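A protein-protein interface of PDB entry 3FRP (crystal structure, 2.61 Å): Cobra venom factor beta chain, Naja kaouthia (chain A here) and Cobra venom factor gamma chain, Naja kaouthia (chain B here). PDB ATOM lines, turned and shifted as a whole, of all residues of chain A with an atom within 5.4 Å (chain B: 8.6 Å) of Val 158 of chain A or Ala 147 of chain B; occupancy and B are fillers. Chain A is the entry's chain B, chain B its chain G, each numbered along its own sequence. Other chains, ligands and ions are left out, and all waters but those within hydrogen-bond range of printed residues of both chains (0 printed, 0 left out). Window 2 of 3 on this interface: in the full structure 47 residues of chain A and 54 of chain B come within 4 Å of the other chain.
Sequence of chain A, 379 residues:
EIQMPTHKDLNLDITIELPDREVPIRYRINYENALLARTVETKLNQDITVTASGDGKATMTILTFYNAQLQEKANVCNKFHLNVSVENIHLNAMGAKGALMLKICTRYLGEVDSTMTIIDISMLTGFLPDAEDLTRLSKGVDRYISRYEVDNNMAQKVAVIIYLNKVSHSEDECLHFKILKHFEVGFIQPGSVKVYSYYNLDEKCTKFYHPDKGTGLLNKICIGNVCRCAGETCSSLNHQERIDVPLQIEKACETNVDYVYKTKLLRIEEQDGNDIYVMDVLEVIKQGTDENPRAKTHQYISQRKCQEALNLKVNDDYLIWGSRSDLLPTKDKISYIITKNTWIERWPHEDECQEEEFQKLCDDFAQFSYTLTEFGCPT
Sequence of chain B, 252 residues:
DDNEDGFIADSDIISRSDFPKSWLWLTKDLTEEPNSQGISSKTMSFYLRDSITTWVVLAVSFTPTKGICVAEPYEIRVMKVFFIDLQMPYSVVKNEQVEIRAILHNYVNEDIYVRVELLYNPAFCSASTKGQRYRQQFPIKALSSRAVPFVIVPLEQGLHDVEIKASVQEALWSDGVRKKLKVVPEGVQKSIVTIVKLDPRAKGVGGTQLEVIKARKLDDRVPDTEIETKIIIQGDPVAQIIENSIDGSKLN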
ATOM      1  N   ILE A 121     -30.519  14.333  19.027  1.00  0.00           N
ATOM      2  CA  ILE A 121     -31.627  13.663  19.720  1.00  0.00           C
ATOM      3  C   ILE A 121     -31.357  12.200  20.146  1.00  0.00           C
ATOM      4  O   ILE A 121     -30.901  11.377  19.340  1.00  0.00           O
ATOM      5  CB  ILE A 121     -32.908  13.651  18.855  1.00  0.00           C
ATOM      6  CG1 ILE A 121     -33.227  15.043  18.306  1.00  0.00           C
ATOM      7  CG2 ILE A 121     -34.077  13.070  19.644  1.00  0.00           C
ATOM      8  CD1 ILE A 121     -34.140  15.016  17.097  1.00  0.00           C
ATOM      9  N   SER A 122     -31.691  11.883  21.396  1.00  0.00           N
ATOM     10  CA  SER A 122     -31.700  10.496  21.884  1.00  0.00           C
ATOM     11  C   SER A 122     -33.126   9.966  22.168  1.00  0.00           C
ATOM     12  O   SER A 122     -34.012  10.704  22.614  1.00  0.00           O
ATOM     13  CB  SER A 122     -30.809  10.353  23.128  1.00  0.00           C
ATOM     14  OG  SER A 122     -31.246  11.210  24.177  1.00  0.00           O
ATOM     15  N   MET A 123     -33.332   8.677  21.916  1.00  0.00           N
ATOM     16  CA  MET A 123     -34.656   8.071  22.072  1.00  0.00           C
ATOM     17  C   MET A 123     -34.908   7.681  23.508  1.00  0.00           C
ATOM     18  O   MET A 123     -33.976   7.352  24.233  1.00  0.00           O
ATOM     19  CB  MET A 123     -34.780   6.840  21.180  1.00  0.00           C
ATOM     20  CG  MET A 123     -34.835   7.155  19.703  1.00  0.00           C
ATOM     21  SD  MET A 123     -36.356   7.972  19.211  1.00  0.00           S
ATOM     22  CE  MET A 123     -35.937   9.702  19.377  1.00  0.00           C
ATOM     23  N   PHE A 127     -37.621   2.838  22.411  1.00  0.00           N
ATOM     24  CA  PHE A 127     -38.354   3.658  21.462  1.00  0.00           C
ATOM     25  C   PHE A 127     -37.529   3.859  20.232  1.00  0.00           C
ATOM     26  O   PHE A 127     -36.295   3.851  20.276  1.00  0.00           O
ATOM     27  CB  PHE A 127     -38.660   5.019  22.045  1.00  0.00           C
ATOM     28  CG  PHE A 127     -39.950   5.084  22.786  1.00  0.00           C
ATOM     29  CD1 PHE A 127     -41.102   5.538  22.155  1.00  0.00           C
ATOM     30  CD2 PHE A 127     -40.019   4.712  24.115  1.00  0.00           C
ATOM     31  CE1 PHE A 127     -42.300   5.622  22.838  1.00  0.00           C
ATOM     32  CE2 PHE A 127     -41.207   4.798  24.805  1.00  0.00           C
ATOM     33  CZ  PHE A 127     -42.353   5.258  24.162  1.00  0.00           C
ATOM     34  N   LEU A 128     -38.221   4.065  19.125  1.00  0.00           N
ATOM     35  CA  LEU A 128     -37.566   4.060  17.851  1.00  0.00           C
ATOM     36  C   LEU A 128     -38.366   4.966  16.940  1.00  0.00           C
ATOM     37  O   LEU A 128     -39.594   5.035  17.054  1.00  0.00           O
ATOM     38  CB  LEU A 128     -37.514   2.621  17.325  1.00  0.00           C
ATOM     39  CG  LEU A 128     -36.241   2.006  16.737  1.00  0.00           C
ATOM     40  CD1 LEU A 128     -35.011   2.179  17.622  1.00  0.00           C
ATOM     41  CD2 LEU A 128     -36.505   0.533  16.487  1.00  0.00           C
ATOM     42  N   GLN A 156     -33.667   2.400  12.419  1.00  0.00           N
ATOM     43  CA  GLN A 156     -32.842   1.642  13.358  1.00  0.00           C
ATOM     44  C   GLN A 156     -31.705   2.493  13.962  1.00  0.00           C
ATOM     45  O   GLN A 156     -30.505   2.260  13.729  1.00  0.00           O
ATOM     46  CB  GLN A 156     -32.364   0.313  12.731  1.00  0.00           C
ATOM     47  CG  GLN A 156     -32.237  -0.848  13.753  1.00  0.00           C
ATOM     48  CD  GLN A 156     -33.580  -1.506  14.153  1.00  0.00           C
ATOM     49  OE1 GLN A 156     -34.669  -1.093  13.714  1.00  0.00           O
ATOM     50  NE2 GLN A 156     -33.492  -2.537  14.995  1.00  0.00           N
ATOM     51  N   LYS A 157     -32.121   3.492  14.740  1.00  0.00           N
ATOM     52  CA  LYS A 157     -31.213   4.447  15.369  1.00  0.00           C
ATOM     53  C   LYS A 157     -31.819   4.994  16.638  1.00  0.00           C
ATOM     54  O   LYS A 157     -32.963   5.453  16.633  1.00  0.00           O
ATOM     55  CB  LYS A 157     -30.840   5.581  14.407  1.00  0.00           C
ATOM     56  CG  LYS A 157     -29.746   5.168  13.438  1.00  0.00           C
ATOM     57  CD  LYS A 157     -28.850   6.284  13.029  1.00  0.00           C
ATOM     58  CE  LYS A 157     -27.608   5.711  12.403  1.00  0.00           C
ATOM     59  NZ  LYS A 157     -26.846   6.768  11.687  1.00  0.00           N
ATOM     60  N   VAL A 158     -31.054   4.920  17.728  1.00  0.00           N
ATOM     61  CA  VAL A 158     -31.499   5.440  19.025  1.00  0.00           C
ATOM     62  C   VAL A 158     -31.028   6.874  19.238  1.00  0.00           C
ATOM     63  O   VAL A 158     -31.705   7.663  19.901  1.00  0.00           O
ATOM     64  CB  VAL A 158     -31.034   4.557  20.186  1.00  0.00           C
ATOM     65  CG1 VAL A 158     -29.554   4.315  20.095  1.00  0.00           C
ATOM     66  CG2 VAL A 158     -31.361   5.197  21.502  1.00  0.00           C
ATOM     67  N   ALA A 159     -29.859   7.194  18.688  1.00  0.00           N
ATOM     68  CA  ALA A 159     -29.374   8.561  18.633  1.00  0.00           C
ATOM     69  C   ALA A 159     -29.526   9.098  17.211  1.00  0.00           C
ATOM     70  O   ALA A 159     -28.806   8.675  16.305  1.00  0.00           O
ATOM     71  CB  ALA A 159     -27.928   8.620  19.069  1.00  0.00           C
ATOM     72  N   VAL A 160     -30.471  10.014  17.021  1.00  0.00           N
ATOM     73  CA  VAL A 160     -30.677  10.666  15.720  1.00  0.00           C
ATOM     74  C   VAL A 160     -30.265  12.138  15.705  1.00  0.00           C
ATOM     75  O   VAL A 160     -30.662  12.932  16.583  1.00  0.00           O
ATOM     76  CB  VAL A 160     -32.136  10.547  15.231  1.00  0.00           C
ATOM     77  CG1 VAL A 160     -33.101  10.870  16.348  1.00  0.00           C
ATOM     78  CG2 VAL A 160     -32.389  11.464  14.038  1.00  0.00           C
ATOM     79  N   ASP B  85     -17.408   1.302  23.965  1.00  0.00           N
ATOM     80  CA  ASP B  85     -16.555   2.488  23.830  1.00  0.00           C
ATOM     81  C   ASP B  85     -17.241   3.630  24.545  1.00  0.00           C
ATOM     82  O   ASP B  85     -18.236   4.173  24.065  1.00  0.00           O
ATOM     83  CB  ASP B  85     -16.274   2.838  22.356  1.00  0.00           C
ATOM     84  CG  ASP B  85     -15.664   4.247  22.174  1.00  0.00           C
ATOM     85  OD1 ASP B  85     -15.967   4.892  21.139  1.00  0.00           O
ATOM     86  OD2 ASP B  85     -14.886   4.710  23.061  1.00  0.00           O
ATOM     87  N   GLU B  99     -26.119  13.352  29.927  1.00  0.00           N
ATOM     88  CA  GLU B  99     -26.287  12.080  29.255  1.00  0.00           C
ATOM     89  C   GLU B  99     -24.958  11.636  28.662  1.00  0.00           C
ATOM     90  O   GLU B  99     -24.298  12.404  27.970  1.00  0.00           O
ATOM     91  CB  GLU B  99     -27.360  12.194  28.177  1.00  0.00           C
ATOM     92  CG  GLU B  99     -27.463  11.014  27.237  1.00  0.00           C
ATOM     93  CD  GLU B  99     -28.475  11.266  26.150  1.00  0.00           C
ATOM     94  OE1 GLU B  99     -28.098  11.312  24.949  1.00  0.00           O
ATOM     95  OE2 GLU B  99     -29.651  11.453  26.503  1.00  0.00           O
ATOM     96  N   ILE B 100     -24.564  10.402  28.953  1.00  0.00           N
ATOM     97  CA  ILE B 100     -23.331   9.840  28.428  1.00  0.00           C
ATOM     98  C   ILE B 100     -23.701   8.742  27.460  1.00  0.00           C
ATOM     99  O   ILE B 100     -24.617   7.960  27.724  1.00  0.00           O
ATOM    100  CB  ILE B 100     -22.446   9.230  29.541  1.00  0.00           C
ATOM    101  CG1 ILE B 100     -22.211  10.219  30.684  1.00  0.00           C
ATOM    102  CG2 ILE B 100     -21.121   8.753  28.977  1.00  0.00           C
ATOM    103  CD1 ILE B 100     -21.761  11.632  30.253  1.00  0.00           C
ATOM    104  N   ARG B 101     -22.980   8.681  26.344  1.00  0.00           N
ATOM    105  CA  ARG B 101     -23.271   7.716  25.296  1.00  0.00           C
ATOM    106  C   ARG B 101     -22.177   6.677  25.127  1.00  0.00           C
ATOM    107  O   ARG B 101     -21.148   6.928  24.487  1.00  0.00           O
ATOM    108  CB  ARG B 101     -23.524   8.434  23.965  1.00  0.00           C
ATOM    109  CG  ARG B 101     -24.752   9.298  23.987  1.00  0.00           C
ATOM    110  CD  ARG B 101     -25.052   9.899  22.632  1.00  0.00           C
ATOM    111  NE  ARG B 101     -26.302  10.644  22.706  1.00  0.00           N
ATOM    112  CZ  ARG B 101     -26.721  11.500  21.793  1.00  0.00           C
ATOM    113  NH1 ARG B 101     -25.985  11.762  20.738  1.00  0.00           N
ATOM    114  NH2 ARG B 101     -27.878  12.125  21.968  1.00  0.00           N
ATOM    115  N   ALA B 102     -22.401   5.503  25.698  1.00  0.00           N
ATOM    116  CA  ALA B 102     -21.585   4.352  25.357  1.00  0.00           C
ATOM    117  C   ALA B 102     -22.024   3.833  23.993  1.00  0.00           C
ATOM    118  O   ALA B 102     -23.210   3.803  23.678  1.00  0.00           O
ATOM    119  CB  ALA B 102     -21.721   3.281  26.391  1.00  0.00           C
ATOM    120  N   ILE B 103     -21.061   3.446  23.176  1.00  0.00           N
ATOM    121  CA  ILE B 103     -21.383   2.823  21.908  1.00  0.00           C
ATOM    122  C   ILE B 103     -20.815   1.411  21.831  1.00  0.00           C
ATOM    123  O   ILE B 103     -19.647   1.165  22.152  1.00  0.00           O
ATOM    124  CB  ILE B 103     -21.027   3.739  20.662  1.00  0.00           C
ATOM    125  CG1 ILE B 103     -20.931   2.917  19.370  1.00  0.00           C
ATOM    126  CG2 ILE B 103     -19.765   4.560  20.900  1.00  0.00           C
ATOM    127  CD1 ILE B 103     -21.380   3.680  18.165  1.00  0.00           C
ATOM    128  N   LEU B 104     -21.691   0.486  21.444  1.00  0.00           N
ATOM    129  CA  LEU B 104     -21.362  -0.926  21.342  1.00  0.00           C
ATOM    130  C   LEU B 104     -20.948  -1.247  19.921  1.00  0.00           C
ATOM    131  O   LEU B 104     -21.599  -0.831  18.973  1.00  0.00           O
ATOM    132  CB  LEU B 104     -22.549  -1.802  21.757  1.00  0.00           C
ATOM    133  CG  LEU B 104     -23.139  -1.631  23.159  1.00  0.00           C
ATOM    134  CD1 LEU B 104     -24.437  -2.397  23.275  1.00  0.00           C
ATOM    135  CD2 LEU B 104     -22.187  -2.095  24.217  1.00  0.00           C
ATOM    136  N   HIS B 105     -19.862  -1.994  19.785  1.00  0.00           N
ATOM    137  CA  HIS B 105     -19.390  -2.419  18.483  1.00  0.00           C
ATOM    138  C   HIS B 105     -19.513  -3.932  18.268  1.00  0.00           C
ATOM    139  O   HIS B 105     -19.037  -4.718  19.081  1.00  0.00           O
ATOM    140  CB  HIS B 105     -17.945  -1.990  18.308  1.00  0.00           C
ATOM    141  CG  HIS B 105     -17.763  -0.515  18.147  1.00  0.00           C
ATOM    142  ND1 HIS B 105     -18.116   0.154  16.996  1.00  0.00           N
ATOM    143  CD2 HIS B 105     -17.227   0.412  18.975  1.00  0.00           C
ATOM    144  CE1 HIS B 105     -17.815   1.434  17.126  1.00  0.00           C
ATOM    145  NE2 HIS B 105     -17.277   1.618  18.319  1.00  0.00           N
ATOM    146  N   VAL B 116     -27.120  -5.164  27.961  1.00  0.00           N
ATOM    147  CA  VAL B 116     -26.315  -4.038  28.402  1.00  0.00           C
ATOM    148  C   VAL B 116     -26.815  -3.537  29.741  1.00  0.00           C
ATOM    149  O   VAL B 116     -27.961  -3.124  29.875  1.00  0.00           O
ATOM    150  CB  VAL B 116     -26.334  -2.873  27.393  1.00  0.00           C
ATOM    151  CG1 VAL B 116     -25.143  -1.977  27.628  1.00  0.00           C
ATOM    152  CG2 VAL B 116     -26.315  -3.393  25.987  1.00  0.00           C
ATOM    153  N   TYR B 134     -30.127  -1.021  35.615  1.00  0.00           N
ATOM    154  CA  TYR B 134     -30.864  -0.707  34.398  1.00  0.00           C
ATOM    155  C   TYR B 134     -30.254  -1.475  33.234  1.00  0.00           C
ATOM    156  O   TYR B 134     -29.215  -1.088  32.690  1.00  0.00           O
ATOM    157  CB  TYR B 134     -30.856   0.811  34.172  1.00  0.00           C
ATOM    158  CG  TYR B 134     -31.085   1.315  32.755  1.00  0.00           C
ATOM    159  CD1 TYR B 134     -32.369   1.360  32.201  1.00  0.00           C
ATOM    160  CD2 TYR B 134     -30.020   1.803  31.990  1.00  0.00           C
ATOM    161  CE1 TYR B 134     -32.583   1.848  30.898  1.00  0.00           C
ATOM    162  CE2 TYR B 134     -30.223   2.294  30.692  1.00  0.00           C
ATOM    163  CZ  TYR B 134     -31.505   2.314  30.156  1.00  0.00           C
ATOM    164  OH  TYR B 134     -31.707   2.796  28.885  1.00  0.00           O
ATOM    165  N   GLN B 136     -30.971  -3.763  29.433  1.00  0.00           N
ATOM    166  CA  GLN B 136     -31.790  -3.749  28.225  1.00  0.00           C
ATOM    167  C   GLN B 136     -31.277  -4.735  27.183  1.00  0.00           C
ATOM    168  O   GLN B 136     -30.075  -4.975  27.063  1.00  0.00           O
ATOM    169  CB  GLN B 136     -31.858  -2.347  27.632  1.00  0.00           C
ATOM    170  CG  GLN B 136     -30.518  -1.659  27.501  1.00  0.00           C
ATOM    171  CD  GLN B 136     -30.627  -0.136  27.498  1.00  0.00           C
ATOM    172  OE1 GLN B 136     -29.724   0.551  27.958  1.00  0.00           O
ATOM    173  NE2 GLN B 136     -31.734   0.392  26.979  1.00  0.00           N
ATOM    174  N   PHE B 138     -31.564  -6.058  23.028  1.00  0.00           N
ATOM    175  CA  PHE B 138     -31.860  -5.601  21.663  1.00  0.00           C
ATOM    176  C   PHE B 138     -30.812  -6.156  20.702  1.00  0.00           C
ATOM    177  O   PHE B 138     -29.745  -6.583  21.143  1.00  0.00           O
ATOM    178  CB  PHE B 138     -31.849  -4.073  21.599  1.00  0.00           C
ATOM    179  CG  PHE B 138     -30.610  -3.461  22.174  1.00  0.00           C
ATOM    180  CD1 PHE B 138     -30.638  -2.862  23.421  1.00  0.00           C
ATOM    181  CD2 PHE B 138     -29.408  -3.498  21.470  1.00  0.00           C
ATOM    182  CE1 PHE B 138     -29.499  -2.303  23.954  1.00  0.00           C
ATOM    183  CE2 PHE B 138     -28.259  -2.948  21.999  1.00  0.00           C
ATOM    184  CZ  PHE B 138     -28.304  -2.344  23.244  1.00  0.00           C
ATOM    185  N   ILE B 140     -28.115  -6.404  17.183  1.00  0.00           N
ATOM    186  CA  ILE B 140     -27.189  -5.630  16.365  1.00  0.00           C
ATOM    187  C   ILE B 140     -26.919  -6.335  15.042  1.00  0.00           C
ATOM    188  O   ILE B 140     -26.611  -7.526  15.010  1.00  0.00           O
ATOM    189  CB  ILE B 140     -25.846  -5.322  17.087  1.00  0.00           C
ATOM    190  CG1 ILE B 140     -26.049  -4.362  18.261  1.00  0.00           C
ATOM    191  CG2 ILE B 140     -24.859  -4.670  16.131  1.00  0.00           C
ATOM    192  CD1 ILE B 140     -26.050  -5.008  19.625  1.00  0.00           C
ATOM    193  N   SER B 144     -21.854  -3.862  12.428  1.00  0.00           N
ATOM    194  CA  SER B 144     -22.428  -2.554  12.772  1.00  0.00           C
ATOM    195  C   SER B 144     -22.319  -2.236  14.256  1.00  0.00           C
ATOM    196  O   SER B 144     -21.725  -3.001  15.020  1.00  0.00           O
ATOM    197  CB  SER B 144     -23.864  -2.401  12.238  1.00  0.00           C
ATOM    198  OG  SER B 144     -24.639  -3.564  12.448  1.00  0.00           O
ATOM    199  N   SER B 145     -22.871  -1.096  14.656  1.00  0.00           N
ATOM    200  CA  SER B 145     -22.729  -0.624  16.033  1.00  0.00           C
ATOM    201  C   SER B 145     -23.987   0.092  16.473  1.00  0.00           C
ATOM    202  O   SER B 145     -24.777   0.529  15.641  1.00  0.00           O
ATOM    203  CB  SER B 145     -21.524   0.307  16.143  1.00  0.00           C
ATOM    204  OG  SER B 145     -21.600   1.293  15.147  1.00  0.00           O
ATOM    205  N   ARG B 146     -24.189   0.206  17.779  1.00  0.00           N
ATOM    206  CA  ARG B 146     -25.395   0.844  18.273  1.00  0.00           C
ATOM    207  C   ARG B 146     -25.143   1.695  19.519  1.00  0.00           C
ATOM    208  O   ARG B 146     -24.531   1.234  20.482  1.00  0.00           O
ATOM    209  CB  ARG B 146     -26.481  -0.212  18.490  1.00  0.00           C
ATOM    210  CG  ARG B 146     -27.905   0.326  18.617  1.00  0.00           C
ATOM    211  CD  ARG B 146     -28.324   0.208  20.060  1.00  0.00           C
ATOM    212  NE  ARG B 146     -29.725  -0.180  20.188  1.00  0.00           N
ATOM    213  CZ  ARG B 146     -30.454   0.026  21.277  1.00  0.00           C
ATOM    214  NH1 ARG B 146     -29.907   0.629  22.330  1.00  0.00           N
ATOM    215  NH2 ARG B 146     -31.726  -0.348  21.306  1.00  0.00           N
ATOM    216  N   ALA B 147     -25.612   2.940  19.483  1.00  0.00           N
ATOM    217  CA  ALA B 147     -25.414   3.872  20.574  1.00  0.00           C
ATOM    218  C   ALA B 147     -26.336   3.528  21.740  1.00  0.00           C
ATOM    219  O   ALA B 147     -27.448   3.071  21.515  1.00  0.00           O
ATOM    220  CB  ALA B 147     -25.674   5.290  20.096  1.00  0.00           C
ATOM    221  N   VAL B 148     -25.859   3.746  22.972  1.00  0.00           N
ATOM    222  CA  VAL B 148     -26.615   3.515  24.213  1.00  0.00           C
ATOM    223  C   VAL B 148     -26.481   4.694  25.208  1.00  0.00           C
ATOM    224  O   VAL B 148     -25.416   4.889  25.825  1.00  0.00           O
ATOM    225  CB  VAL B 148     -26.170   2.207  24.955  1.00  0.00           C
ATOM    226  CG1 VAL B 148     -27.144   1.882  26.063  1.00  0.00           C
ATOM    227  CG2 VAL B 148     -26.061   1.029  24.011  1.00  0.00           C
ATOM    228  N   PRO B 149     -27.561   5.461  25.393  1.00  0.00           N
ATOM    229  CA  PRO B 149     -27.539   6.616  26.296  1.00  0.00           C
ATOM    230  C   PRO B 149     -27.765   6.259  27.750  1.00  0.00           C
ATOM    231  O   PRO B 149     -28.622   5.429  28.057  1.00  0.00           O
ATOM    232  CB  PRO B 149     -28.726   7.449  25.815  1.00  0.00           C
ATOM    233  CG  PRO B 149     -29.685   6.415  25.255  1.00  0.00           C
ATOM    234  CD  PRO B 149     -28.802   5.389  24.608  1.00  0.00           C
ATOM    235  N   PHE B 150     -27.022   6.910  28.641  1.00  0.00           N
ATOM    236  CA  PHE B 150     -27.265   6.816  30.082  1.00  0.00           C
ATOM    237  C   PHE B 150     -27.376   8.201  30.694  1.00  0.00           C
ATOM    238  O   PHE B 150     -26.497   9.027  30.494  1.00  0.00           O
ATOM    239  CB  PHE B 150     -26.132   6.056  30.757  1.00  0.00           C
ATOM    240  CG  PHE B 150     -25.976   4.651  30.267  1.00  0.00           C
ATOM    241  CD1 PHE B 150     -26.837   3.648  30.706  1.00  0.00           C
ATOM    242  CD2 PHE B 150     -24.976   4.324  29.369  1.00  0.00           C
ATOM    243  CE1 PHE B 150     -26.712   2.355  30.250  1.00  0.00           C
ATOM    244  CE2 PHE B 150     -24.835   3.039  28.925  1.00  0.00           C
ATOM    245  CZ  PHE B 150     -25.715   2.049  29.366  1.00  0.00           C
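Printed residues of chain B within 4 Å of Val 158 of chain A: Ala 147 (2.8 Å). Ala 147 of chain B touches just one residue of chain A: Val 158 (2.8 Å). No residue of chain B comes within 4 Å of Ala 159 of chain A. Printed residues of chain A within 4 Å of Glu 99 of chain B: Ser 122 (2.8 Å). Of the printed residues of chain A, Arg 101 of chain B touches Ile 121 (3.9 Å) and Ser 122 (3.6 Å). Of the printed residues of chain B, Ile 121 of chain A touches Arg 101. Printed residues of chain B within 4 Å of Ser 122 of chain A: Glu 99 (2.8 Å) and Arg 101 (3.6 Å). Pro 149 of chain B touches none of the printed residues of chain A. Lys 157 of chain A touches none of the printed residues of chain B. The nearest residue of chain B that does not touch Val 158 of chain A is Pro 149 of chain B (4.03 Å). The nearest residue of chain A that does not touch Ala 147 of chain B is Ala 159 of chain A (4.2 Å).
Arg 101 of chain B touches Ile 121 of chain A (NH2 to C, 3.9 Å). Ser 122 of chain A touches Arg 101 of chain B. CG1 of Val 158 of chain A touches O of Ala 147 of chain B, at 2.8 Å.
OE1 of Glu 99 of chain B lies within salt-bridge range of NE of Arg 101 of chain B, 3.0 Å away. The backbone carbonyl oxygen (O) of Ile 121 of chain A is in hydrogen-bond range of the backbone NH (N) of Val 160 of chain A (2.7 Å). N of Met 123 of chain A is in hydrogen-bond range of O of Val 158 of chain A (2.8 Å).
The side-chain carboxylate (OE2) of Glu 99 of chain B is in hydrogen-bond range of the side-chain hydroxyl (OG) of Ser 122 of chain A, at 2.8 Å.
Of the 20 printed residues of chain B, 3 touch a printed residue of chain A. Of the 10 printed residues of chain A, 3 touch a printed residue of chain B. Among the printed residues, no Asp or Glu carboxylate lies within 4 Å of a Lys or Arg side-chain nitrogen of the other chain.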
